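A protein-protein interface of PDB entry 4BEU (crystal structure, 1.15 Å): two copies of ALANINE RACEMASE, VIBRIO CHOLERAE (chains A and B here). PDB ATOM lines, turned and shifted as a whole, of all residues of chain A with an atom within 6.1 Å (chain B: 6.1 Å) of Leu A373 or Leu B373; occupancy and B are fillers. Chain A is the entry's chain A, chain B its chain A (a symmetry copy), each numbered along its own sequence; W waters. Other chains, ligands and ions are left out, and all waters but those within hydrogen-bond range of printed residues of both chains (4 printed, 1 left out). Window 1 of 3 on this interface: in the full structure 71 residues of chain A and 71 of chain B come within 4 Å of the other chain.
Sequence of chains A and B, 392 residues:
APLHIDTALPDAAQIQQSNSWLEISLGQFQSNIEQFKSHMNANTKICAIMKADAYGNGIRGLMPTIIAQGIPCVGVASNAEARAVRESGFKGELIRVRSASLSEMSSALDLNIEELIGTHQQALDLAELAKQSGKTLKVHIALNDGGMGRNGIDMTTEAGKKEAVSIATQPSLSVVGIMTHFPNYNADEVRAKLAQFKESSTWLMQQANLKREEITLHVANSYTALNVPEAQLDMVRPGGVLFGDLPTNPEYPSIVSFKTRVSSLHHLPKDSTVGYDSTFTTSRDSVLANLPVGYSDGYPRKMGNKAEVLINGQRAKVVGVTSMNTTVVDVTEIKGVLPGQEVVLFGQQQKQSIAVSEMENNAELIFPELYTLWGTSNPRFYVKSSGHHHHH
Of chain A, only Tyr A295 (3.7 Å), Ser A296 (3.4 Å), Leu A373 (3.7 Å) and Ser A377 (3.5 Å) come within 4 Å of Leu B373.
Of the printed residues of chain B, Pro A368 touches Tyr B295.
Of the printed residues of chain A, Ser B296 touches Thr A372 and Leu A373.
Printed residues of chain A within 4 Å of Pro B368: Tyr A295.
Of the printed residues of chain B, Tyr A295 touches Pro B368, Glu B369, Thr B372 and Leu B373.
Gly B56 touches none of the printed residues of chain A.
Asn A378 touches none of the printed residues of chain B.
The side-chain hydroxyl (OG) of Ser B377 lies within hydrogen-bond range of the side-chain hydroxyl (OG1) of Thr A376 (2.8 Å).
The side-chain hydroxyl of Thr B376 lies within hydrogen-bond range of the side-chain hydroxyl of Ser A377 (2.8 Å).
The backbone carbonyl oxygen (O) of Thr A376 sits close to the backbone carbonyl oxygen (O) of Thr B376 (3.4 Å).
Tyr A295 touches Glu B369, and with the chains exchanged Glu A369 touches Tyr B295.
Ser A296 touches Leu B373, and with the chains exchanged Leu A373 touches Ser B296.
Thr B376 touches its own counterpart, Thr A376.
Thr A376 touches Ser B377, and with the chains exchanged Ser A377 touches Thr B376.
Positions printed for both chains: 56, 295, 296, 297, 298, 368, 369, 370, 371, 372, 373, 374, 375, 376, 377 and 378.
Water W3 bridges the backbone carbonyl oxygen of Ser A296 and the backbone carbonyl oxygen of Thr B372.
Water W1 lies within hydrogen-bond range of the backbone carbonyl oxygen (O) of Ser B296 (2.6 Å) and the backbone carbonyl oxygen (O) of Thr A372 (3.0 Å).
Water W4 bridges the backbone carbonyl oxygen (O) of Glu A369 (2.8 Å) and the backbone carbonyl oxygen (O) of Tyr B295 (2.9 Å).
Water W2 bridges O of Glu B369 (2.8 Å) and O of Tyr A295 (2.9 Å).
Among the printed residues, pairs that only touch across the chains: Tyr A295 with Pro B368 (3.4 Å), Tyr A295 with Glu B369 (3.8 Å), Tyr A295 with Thr B372 (3.96 Å), Tyr A295 with Leu B373 (3.7 Å), Ser A296 with Thr B372 (3.6 Å), Ser A296 with Leu B373 (3.4 Å), Pro A368 with Tyr B295 (3.4 Å), Glu A369 with Tyr B295 (3.8 Å), Thr A372 with Tyr B295 (3.96 Å), Thr A372 with Ser B296 (3.6 Å), Leu A373 with Tyr B295 (3.7 Å), Leu A373 with Ser B296 (3.4 Å), Leu A373 with Leu B373 (3.7 Å), Leu A373 with Ser B377 (3.5 Å) and Ser A377 with Leu B373 (3.5 Å).
Hydrophobic or aromatic side chains of chain A within 4 Å of the printed part of chain B: Tyr A295, Pro A368 and Leu A373.
The backbone carbonyl oxygen of Pro A368 lies within hydrogen-bond range of the side-chain hydroxyl of Thr A372, 2.8 Å away.
O of Leu A373 sits at hydrogen-bond distance from OG of Ser A377, at 2.8 Å.
The side-chain hydroxyl of Thr A376 lies within hydrogen-bond range of the side-chain hydroxyl of Ser A377 (3.3 Å).
The backbone carbonyl oxygen (O) of Leu B373 sits at hydrogen-bond distance from the side-chain hydroxyl (OG1) of Thr B376, 3.1 Å away.
OG of Ser B377 is in hydrogen-bond range of O of Leu B373 (2.8 Å).
OG1 of Thr B376 lies within hydrogen-bond range of OG of Ser B377.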
ATOM      1  N   GLY A  56      -9.716  23.652 -33.011  1.00  0.00           N
ATOM      2  CA  GLY A  56      -9.952  22.254 -33.297  1.00  0.00           C
ATOM      3  C   GLY A  56     -10.142  21.928 -34.758  1.00  0.00           C
ATOM      4  O   GLY A  56     -10.148  20.745 -35.128  1.00  0.00           O
ATOM      5  N   TYR A 295     -15.088   8.427 -24.672  1.00  0.00           N
ATOM      6  CA  TYR A 295     -14.618   9.664 -24.073  1.00  0.00           C
ATOM      7  C   TYR A 295     -13.158   9.973 -24.389  1.00  0.00           C
ATOM      8  O   TYR A 295     -12.769  11.134 -24.371  1.00  0.00           O
ATOM      9  CB  TYR A 295     -14.932   9.743 -22.564  1.00  0.00           C
ATOM     10  CG  TYR A 295     -14.329   8.686 -21.670  1.00  0.00           C
ATOM     11  CD1 TYR A 295     -12.978   8.669 -21.399  1.00  0.00           C
ATOM     12  CD2 TYR A 295     -15.145   7.737 -21.046  1.00  0.00           C
ATOM     13  CE1 TYR A 295     -12.428   7.709 -20.575  1.00  0.00           C
ATOM     14  CE2 TYR A 295     -14.608   6.785 -20.207  1.00  0.00           C
ATOM     15  CZ  TYR A 295     -13.249   6.777 -19.978  1.00  0.00           C
ATOM     16  OH  TYR A 295     -12.665   5.848 -19.152  1.00  0.00           O
ATOM     17  N   SER A 296     -12.364   8.967 -24.738  1.00  0.00           N
ATOM     18  CA  SER A 296     -10.998   9.247 -25.177  1.00  0.00           C
ATOM     19  C   SER A 296     -10.927   9.891 -26.557  1.00  0.00           C
ATOM     20  O   SER A 296      -9.875  10.414 -26.937  1.00  0.00           O
ATOM     21  CB  SER A 296     -10.130   7.992 -25.129  1.00  0.00           C
ATOM     22  OG  SER A 296     -10.498   7.036 -26.094  1.00  0.00           O
ATOM     23  N   ASP A 297     -12.048   9.898 -27.283  1.00  0.00           N
ATOM     24  CA  ASP A 297     -12.158  10.639 -28.544  1.00  0.00           C
ATOM     25  C   ASP A 297     -12.794  12.018 -28.331  1.00  0.00           C
ATOM     26  O   ASP A 297     -12.957  12.779 -29.281  1.00  0.00           O
ATOM     27  CB  ASP A 297     -13.002   9.859 -29.543  1.00  0.00           C
ATOM     28  CG  ASP A 297     -12.536   8.444 -29.686  1.00  0.00           C
ATOM     29  OD1 ASP A 297     -11.443   8.248 -30.265  1.00  0.00           O
ATOM     30  OD2 ASP A 297     -13.236   7.515 -29.211  1.00  0.00           O
ATOM     31  N   GLY A 298     -13.191  12.317 -27.092  1.00  0.00           N
ATOM     32  CA  GLY A 298     -13.846  13.571 -26.764  1.00  0.00           C
ATOM     33  C   GLY A 298     -15.365  13.517 -26.757  1.00  0.00           C
ATOM     34  O   GLY A 298     -16.007  14.575 -26.792  1.00  0.00           O
ATOM     35  N   PRO A 368     -16.635  25.195 -26.839  1.00  0.00           N
ATOM     36  CA  PRO A 368     -15.200  25.102 -27.174  1.00  0.00           C
ATOM     37  C   PRO A 368     -14.437  24.086 -26.330  1.00  0.00           C
ATOM     38  O   PRO A 368     -13.380  23.589 -26.750  1.00  0.00           O
ATOM     39  CB  PRO A 368     -14.677  26.530 -26.944  1.00  0.00           C
ATOM     40  CG  PRO A 368     -15.737  27.244 -26.187  1.00  0.00           C
ATOM     41  CD  PRO A 368     -17.038  26.569 -26.488  1.00  0.00           C
ATOM     42  N   GLU A 369     -14.918  23.784 -25.139  1.00  0.00           N
ATOM     43  CA  GLU A 369     -14.279  22.716 -24.364  1.00  0.00           C
ATOM     44  C   GLU A 369     -14.395  21.384 -25.083  1.00  0.00           C
ATOM     45  O   GLU A 369     -13.486  20.544 -24.987  1.00  0.00           O
ATOM     46  CB  GLU A 369     -14.884  22.576 -22.978  1.00  0.00           C
ATOM     47  CG  GLU A 369     -14.513  23.667 -22.022  1.00  0.00           C
ATOM     48  CD  GLU A 369     -15.114  23.425 -20.663  1.00  0.00           C
ATOM     49  OE1 GLU A 369     -16.320  23.718 -20.501  1.00  0.00           O
ATOM     50  OE2 GLU A 369     -14.396  22.932 -19.783  1.00  0.00           O
ATOM     51  N   LEU A 370     -15.509  21.167 -25.765  1.00  0.00           N
ATOM     52  CA  LEU A 370     -15.687  19.976 -26.572  1.00  0.00           C
ATOM     53  C   LEU A 370     -14.819  20.017 -27.819  1.00  0.00           C
ATOM     54  O   LEU A 370     -14.007  19.102 -28.045  1.00  0.00           O
ATOM     55  CB  LEU A 370     -17.154  19.818 -26.961  1.00  0.00           C
ATOM     56  CG  LEU A 370     -18.075  19.346 -25.833  1.00  0.00           C
ATOM     57  CD1 LEU A 370     -19.527  19.660 -26.197  1.00  0.00           C
ATOM     58  CD2 LEU A 370     -17.903  17.862 -25.586  1.00  0.00           C
ATOM     59  N   TYR A 371     -14.962  21.057 -28.641  1.00  0.00           N
ATOM     60  CA  TYR A 371     -14.364  20.978 -29.964  1.00  0.00           C
ATOM     61  C   TYR A 371     -12.851  21.140 -29.965  1.00  0.00           C
ATOM     62  O   TYR A 371     -12.184  20.591 -30.860  1.00  0.00           O
ATOM     63  CB  TYR A 371     -15.064  21.899 -30.975  1.00  0.00           C
ATOM     64  CG  TYR A 371     -15.071  23.397 -30.736  1.00  0.00           C
ATOM     65  CD1 TYR A 371     -13.899  24.130 -30.691  1.00  0.00           C
ATOM     66  CD2 TYR A 371     -16.278  24.092 -30.618  1.00  0.00           C
ATOM     67  CE1 TYR A 371     -13.929  25.510 -30.538  1.00  0.00           C
ATOM     68  CE2 TYR A 371     -16.307  25.467 -30.480  1.00  0.00           C
ATOM     69  CZ  TYR A 371     -15.137  26.158 -30.437  1.00  0.00           C
ATOM     70  OH  TYR A 371     -15.119  27.525 -30.294  1.00  0.00           O
ATOM     71  N   THR A 372     -12.285  21.835 -28.984  1.00  0.00           N
ATOM     72  CA  THR A 372     -10.834  21.922 -28.982  1.00  0.00           C
ATOM     73  C   THR A 372     -10.197  20.554 -28.735  1.00  0.00           C
ATOM     74  O   THR A 372      -9.161  20.215 -29.338  1.00  0.00           O
ATOM     75  CB  THR A 372     -10.286  22.951 -27.991  1.00  0.00           C
ATOM     76  OG1 THR A 372     -10.716  22.674 -26.667  1.00  0.00           O
ATOM     77  CG2 THR A 372     -10.662  24.360 -28.427  1.00  0.00           C
ATOM     78  N   LEU A 373     -10.815  19.736 -27.895  1.00  0.00           N
ATOM     79  CA  LEU A 373     -10.287  18.402 -27.614  1.00  0.00           C
ATOM     80  C   LEU A 373     -10.725  17.411 -28.691  1.00  0.00           C
ATOM     81  O   LEU A 373     -10.021  16.430 -28.964  1.00  0.00           O
ATOM     82  CB  LEU A 373     -10.645  17.946 -26.189  1.00  0.00           C
ATOM     83  CG  LEU A 373     -10.096  18.874 -25.110  1.00  0.00           C
ATOM     84  CD1 LEU A 373     -10.469  18.374 -23.722  1.00  0.00           C
ATOM     85  CD2 LEU A 373      -8.602  19.063 -25.217  1.00  0.00           C
ATOM     86  N   TRP A 374     -11.861  17.642 -29.342  1.00  0.00           N
ATOM     87  CA  TRP A 374     -12.140  16.845 -30.546  1.00  0.00           C
ATOM     88  C   TRP A 374     -10.975  16.971 -31.517  1.00  0.00           C
ATOM     89  O   TRP A 374     -10.565  15.998 -32.163  1.00  0.00           O
ATOM     90  CB  TRP A 374     -13.412  17.293 -31.253  1.00  0.00           C
ATOM     91  CG  TRP A 374     -14.686  17.070 -30.550  1.00  0.00           C
ATOM     92  CD1 TRP A 374     -14.903  16.284 -29.464  1.00  0.00           C
ATOM     93  CD2 TRP A 374     -15.943  17.654 -30.878  1.00  0.00           C
ATOM     94  NE1 TRP A 374     -16.216  16.348 -29.082  1.00  0.00           N
ATOM     95  CE2 TRP A 374     -16.878  17.171 -29.950  1.00  0.00           C
ATOM     96  CE3 TRP A 374     -16.372  18.543 -31.865  1.00  0.00           C
ATOM     97  CZ2 TRP A 374     -18.223  17.548 -29.978  1.00  0.00           C
ATOM     98  CZ3 TRP A 374     -17.712  18.917 -31.895  1.00  0.00           C
ATOM     99  CH2 TRP A 374     -18.612  18.423 -30.949  1.00  0.00           C
ATOM    100  N   GLY A 375     -10.474  18.180 -31.671  1.00  0.00           N
ATOM    101  CA  GLY A 375      -9.452  18.438 -32.660  1.00  0.00           C
ATOM    102  C   GLY A 375      -8.087  17.867 -32.333  1.00  0.00           C
ATOM    103  O   GLY A 375      -7.318  17.589 -33.266  1.00  0.00           O
ATOM    104  N   THR A 376      -7.740  17.702 -31.064  1.00  0.00           N
ATOM    105  CA  THR A 376      -6.485  17.035 -30.729  1.00  0.00           C
ATOM    106  C   THR A 376      -6.618  15.509 -30.791  1.00  0.00           C
ATOM    107  O   THR A 376      -5.605  14.818 -30.771  1.00  0.00           O
ATOM    108  CB  THR A 376      -5.985  17.402 -29.337  1.00  0.00           C
ATOM    109  OG1 THR A 376      -7.008  17.075 -28.405  1.00  0.00           O
ATOM    110  CG2 THR A 376      -5.651  18.883 -29.225  1.00  0.00           C
ATOM    111  N   SER A 377      -7.842  14.987 -30.850  1.00  0.00           N
ATOM    112  CA  SER A 377      -8.077  13.567 -30.626  1.00  0.00           C
ATOM    113  C   SER A 377      -8.673  12.835 -31.821  1.00  0.00           C
ATOM    114  O   SER A 377      -8.955  11.638 -31.721  1.00  0.00           O
ATOM    115  CB  SER A 377      -8.990  13.380 -29.415  1.00  0.00           C
ATOM    116  OG  SER A 377      -8.543  14.139 -28.298  1.00  0.00           O
ATOM    117  N   ASN A 378      -8.852  13.521 -32.954  1.00  0.00           N
ATOM    118  CA  ASN A 378      -9.463  12.939 -34.144  1.00  0.00           C
ATOM    119  C   ASN A 378      -8.914  13.595 -35.386  1.00  0.00           C
ATOM    120  O   ASN A 378      -8.606  14.794 -35.373  1.00  0.00           O
ATOM    121  CB  ASN A 378     -10.972  13.185 -34.141  1.00  0.00           C
ATOM    122  CG  ASN A 378     -11.655  12.566 -32.953  1.00  0.00           C
ATOM    123  OD1 ASN A 378     -11.940  11.366 -32.947  1.00  0.00           O
ATOM    124  ND2 ASN A 378     -11.905  13.365 -31.944  1.00  0.00           N
ATOM    125  N   GLY B  56      -3.361   7.504 -22.226  1.00  0.00           N
ATOM    126  CA  GLY B  56      -2.767   8.822 -22.271  1.00  0.00           C
ATOM    127  C   GLY B  56      -1.281   8.857 -22.009  1.00  0.00           C
ATOM    128  O   GLY B  56      -0.644   9.899 -22.222  1.00  0.00           O
ATOM    129  N   TYR B 295      -8.140  25.005 -21.177  1.00  0.00           N
ATOM    130  CA  TYR B 295      -8.989  23.853 -21.426  1.00  0.00           C
ATOM    131  C   TYR B 295      -8.683  23.148 -22.743  1.00  0.00           C
ATOM    132  O   TYR B 295      -8.953  21.961 -22.870  1.00  0.00           O
ATOM    133  CB  TYR B 295     -10.488  24.180 -21.258  1.00  0.00           C
ATOM    134  CG  TYR B 295     -11.076  25.234 -22.165  1.00  0.00           C
ATOM    135  CD1 TYR B 295     -11.268  24.991 -23.508  1.00  0.00           C
ATOM    136  CD2 TYR B 295     -11.499  26.461 -21.644  1.00  0.00           C
ATOM    137  CE1 TYR B 295     -11.815  25.951 -24.335  1.00  0.00           C
ATOM    138  CE2 TYR B 295     -12.064  27.419 -22.458  1.00  0.00           C
ATOM    139  CZ  TYR B 295     -12.216  27.157 -23.802  1.00  0.00           C
ATOM    140  OH  TYR B 295     -12.770  28.079 -24.655  1.00  0.00           O
ATOM    141  N   SER B 296      -8.067  23.838 -23.697  1.00  0.00           N
ATOM    142  CA  SER B 296      -7.639  23.156 -24.917  1.00  0.00           C
ATOM    143  C   SER B 296      -6.448  22.229 -24.705  1.00  0.00           C
ATOM    144  O   SER B 296      -6.150  21.403 -25.573  1.00  0.00           O
ATOM    145  CB  SER B 296      -7.348  24.151 -26.038  1.00  0.00           C
ATOM    146  OG  SER B 296      -6.204  24.933 -25.790  1.00  0.00           O
ATOM    147  N   ASP B 297      -5.801  22.328 -23.541  1.00  0.00           N
ATOM    148  CA  ASP B 297      -4.757  21.377 -23.144  1.00  0.00           C
ATOM    149  C   ASP B 297      -5.319  20.268 -22.248  1.00  0.00           C
ATOM    150  O   ASP B 297      -4.584  19.378 -21.827  1.00  0.00           O
ATOM    151  CB  ASP B 297      -3.645  22.097 -22.392  1.00  0.00           C
ATOM    152  CG  ASP B 297      -3.150  23.297 -23.137  1.00  0.00           C
ATOM    153  OD1 ASP B 297      -2.488  23.100 -24.183  1.00  0.00           O
ATOM    154  OD2 ASP B 297      -3.427  24.445 -22.709  1.00  0.00           O
ATOM    155  N   GLY B 298      -6.611  20.347 -21.925  1.00  0.00           N
ATOM    156  CA  GLY B 298      -7.258  19.385 -21.050  1.00  0.00           C
ATOM    157  C   GLY B 298      -7.327  19.795 -19.588  1.00  0.00           C
ATOM    158  O   GLY B 298      -7.574  18.936 -18.731  1.00  0.00           O
ATOM    159  N   PRO B 368     -10.058   9.014 -15.805  1.00  0.00           N
ATOM    160  CA  PRO B 368      -9.640   8.691 -17.184  1.00  0.00           C
ATOM    161  C   PRO B 368     -10.183   9.658 -18.232  1.00  0.00           C
ATOM    162  O   PRO B 368      -9.606   9.789 -19.324  1.00  0.00           O
ATOM    163  CB  PRO B 368     -10.173   7.266 -17.405  1.00  0.00           C
ATOM    164  CG  PRO B 368     -11.129   7.004 -16.298  1.00  0.00           C
ATOM    165  CD  PRO B 368     -10.742   7.883 -15.151  1.00  0.00           C
ATOM    166  N   GLU B 369     -11.291  10.317 -17.953  1.00  0.00           N
ATOM    167  CA  GLU B 369     -11.761  11.346 -18.885  1.00  0.00           C
ATOM    168  C   GLU B 369     -10.755  12.479 -18.989  1.00  0.00           C
ATOM    169  O   GLU B 369     -10.605  13.082 -20.063  1.00  0.00           O
ATOM    170  CB  GLU B 369     -13.103  11.923 -18.470  1.00  0.00           C
ATOM    171  CG  GLU B 369     -14.269  11.011 -18.690  1.00  0.00           C
ATOM    172  CD  GLU B 369     -15.561  11.677 -18.299  1.00  0.00           C
ATOM    173  OE1 GLU B 369     -15.847  11.718 -17.081  1.00  0.00           O
ATOM    174  OE2 GLU B 369     -16.264  12.167 -19.193  1.00  0.00           O
ATOM    175  N   LEU B 370     -10.097  12.799 -17.884  1.00  0.00           N
ATOM    176  CA  LEU B 370      -9.043  13.793 -17.888  1.00  0.00           C
ATOM    177  C   LEU B 370      -7.798  13.278 -18.594  1.00  0.00           C
ATOM    178  O   LEU B 370      -7.324  13.905 -19.558  1.00  0.00           O
ATOM    179  CB  LEU B 370      -8.700  14.202 -16.459  1.00  0.00           C
ATOM    180  CG  LEU B 370      -9.729  15.112 -15.783  1.00  0.00           C
ATOM    181  CD1 LEU B 370      -9.522  15.077 -14.268  1.00  0.00           C
ATOM    182  CD2 LEU B 370      -9.612  16.531 -16.298  1.00  0.00           C
ATOM    183  N   TYR B 371      -7.253  12.148 -18.145  1.00  0.00           N
ATOM    184  CA  TYR B 371      -5.920  11.794 -18.608  1.00  0.00           C
ATOM    185  C   TYR B 371      -5.882  11.284 -20.040  1.00  0.00           C
ATOM    186  O   TYR B 371      -4.851  11.452 -20.716  1.00  0.00           O
ATOM    187  CB  TYR B 371      -5.190  10.867 -17.624  1.00  0.00           C
ATOM    188  CG  TYR B 371      -5.775   9.501 -17.316  1.00  0.00           C
ATOM    189  CD1 TYR B 371      -5.933   8.541 -18.298  1.00  0.00           C
ATOM    190  CD2 TYR B 371      -6.113   9.152 -16.004  1.00  0.00           C
ATOM    191  CE1 TYR B 371      -6.408   7.274 -17.984  1.00  0.00           C
ATOM    192  CE2 TYR B 371      -6.572   7.887 -15.691  1.00  0.00           C
ATOM    193  CZ  TYR B 371      -6.718   6.966 -16.681  1.00  0.00           C
ATOM    194  OH  TYR B 371      -7.178   5.699 -16.416  1.00  0.00           O
ATOM    195  N   THR B 372      -6.970  10.706 -20.539  1.00  0.00           N
ATOM    196  CA  THR B 372      -6.920  10.283 -21.929  1.00  0.00           C
ATOM    197  C   THR B 372      -6.807  11.483 -22.871  1.00  0.00           C
ATOM    198  O   THR B 372      -6.091  11.429 -23.888  1.00  0.00           O
ATOM    199  CB  THR B 372      -8.097   9.395 -22.339  1.00  0.00           C
ATOM    200  OG1 THR B 372      -9.339  10.046 -22.117  1.00  0.00           O
ATOM    201  CG2 THR B 372      -8.024   8.054 -21.623  1.00  0.00           C
ATOM    202  N   LEU B 373      -7.461  12.586 -22.535  1.00  0.00           N
ATOM    203  CA  LEU B 373      -7.393  13.786 -23.366  1.00  0.00           C
ATOM    204  C   LEU B 373      -6.136  14.593 -23.046  1.00  0.00           C
ATOM    205  O   LEU B 373      -5.606  15.298 -23.915  1.00  0.00           O
ATOM    206  CB  LEU B 373      -8.687  14.612 -23.264  1.00  0.00           C
ATOM    207  CG  LEU B 373      -9.925  13.839 -23.704  1.00  0.00           C
ATOM    208  CD1 LEU B 373     -11.174  14.702 -23.593  1.00  0.00           C
ATOM    209  CD2 LEU B 373      -9.792  13.285 -25.102  1.00  0.00           C
ATOM    210  N   TRP B 374      -5.615  14.501 -21.826  1.00  0.00           N
ATOM    211  CA  TRP B 374      -4.272  15.059 -21.606  1.00  0.00           C
ATOM    212  C   TRP B 374      -3.302  14.454 -22.610  1.00  0.00           C
ATOM    213  O   TRP B 374      -2.426  15.139 -23.153  1.00  0.00           O
ATOM    214  CB  TRP B 374      -3.755  14.780 -20.201  1.00  0.00           C
ATOM    215  CG  TRP B 374      -4.448  15.444 -19.085  1.00  0.00           C
ATOM    216  CD1 TRP B 374      -5.328  16.476 -19.157  1.00  0.00           C
ATOM    217  CD2 TRP B 374      -4.329  15.116 -17.705  1.00  0.00           C
ATOM    218  NE1 TRP B 374      -5.779  16.808 -17.908  1.00  0.00           N
ATOM    219  CE2 TRP B 374      -5.162  15.995 -16.997  1.00  0.00           C
ATOM    220  CE3 TRP B 374      -3.601  14.160 -16.994  1.00  0.00           C
ATOM    221  CZ2 TRP B 374      -5.291  15.948 -15.606  1.00  0.00           C
ATOM    222  CZ3 TRP B 374      -3.726  14.114 -15.609  1.00  0.00           C
ATOM    223  CH2 TRP B 374      -4.574  14.999 -14.939  1.00  0.00           C
ATOM    224  N   GLY B 375      -3.412  13.157 -22.818  1.00  0.00           N
ATOM    225  CA  GLY B 375      -2.462  12.458 -23.653  1.00  0.00           C
ATOM    226  C   GLY B 375      -2.578  12.749 -25.135  1.00  0.00           C
ATOM    227  O   GLY B 375      -1.568  12.628 -25.847  1.00  0.00           O
ATOM    228  N   THR B 376      -3.754  13.099 -25.638  1.00  0.00           N
ATOM    229  CA  THR B 376      -3.859  13.509 -27.035  1.00  0.00           C
ATOM    230  C   THR B 376      -3.447  14.972 -27.232  1.00  0.00           C
ATOM    231  O   THR B 376      -3.253  15.392 -28.367  1.00  0.00           O
ATOM    232  CB  THR B 376      -5.272  13.347 -27.583  1.00  0.00           C
ATOM    233  OG1 THR B 376      -6.150  14.099 -26.756  1.00  0.00           O
ATOM    234  CG2 THR B 376      -5.713  11.890 -27.596  1.00  0.00           C
ATOM    235  N   SER B 377      -3.327  15.741 -26.151  1.00  0.00           N
ATOM    236  CA  SER B 377      -3.222  17.190 -26.254  1.00  0.00           C
ATOM    237  C   SER B 377      -1.919  17.764 -25.714  1.00  0.00           C
ATOM    238  O   SER B 377      -1.749  18.986 -25.711  1.00  0.00           O
ATOM    239  CB  SER B 377      -4.399  17.846 -25.534  1.00  0.00           C
ATOM    240  OG  SER B 377      -5.640  17.265 -25.917  1.00  0.00           O
ATOM    241  N   ASN B 378      -0.990  16.910 -25.275  1.00  0.00           N
ATOM    242  CA  ASN B 378       0.272  17.346 -24.686  1.00  0.00           C
ATOM    243  C   ASN B 378       1.350  16.326 -24.949  1.00  0.00           C
ATOM    244  O   ASN B 378       1.071  15.120 -24.989  1.00  0.00           O
ATOM    245  CB  ASN B 378       0.136  17.468 -23.168  1.00  0.00           C
ATOM    246  CG  ASN B 378      -0.905  18.474 -22.762  1.00  0.00           C
ATOM    247  OD1 ASN B 378      -0.643  19.679 -22.747  1.00  0.00           O
ATOM    248  ND2 ASN B 378      -2.085  17.996 -22.449  1.00  0.00           N
HETATM  249  O   HOH W   1      -6.844  21.595 -28.115  1.00  0.00           O
HETATM  250  O   HOH W   2     -12.675  12.325 -21.779  1.00  0.00           O
HETATM  251  O   HOH W   3      -7.487   9.842 -25.961  1.00  0.00           O
HETATM  252  O   HOH W   4     -11.745  21.375 -22.967  1.00  0.00           O
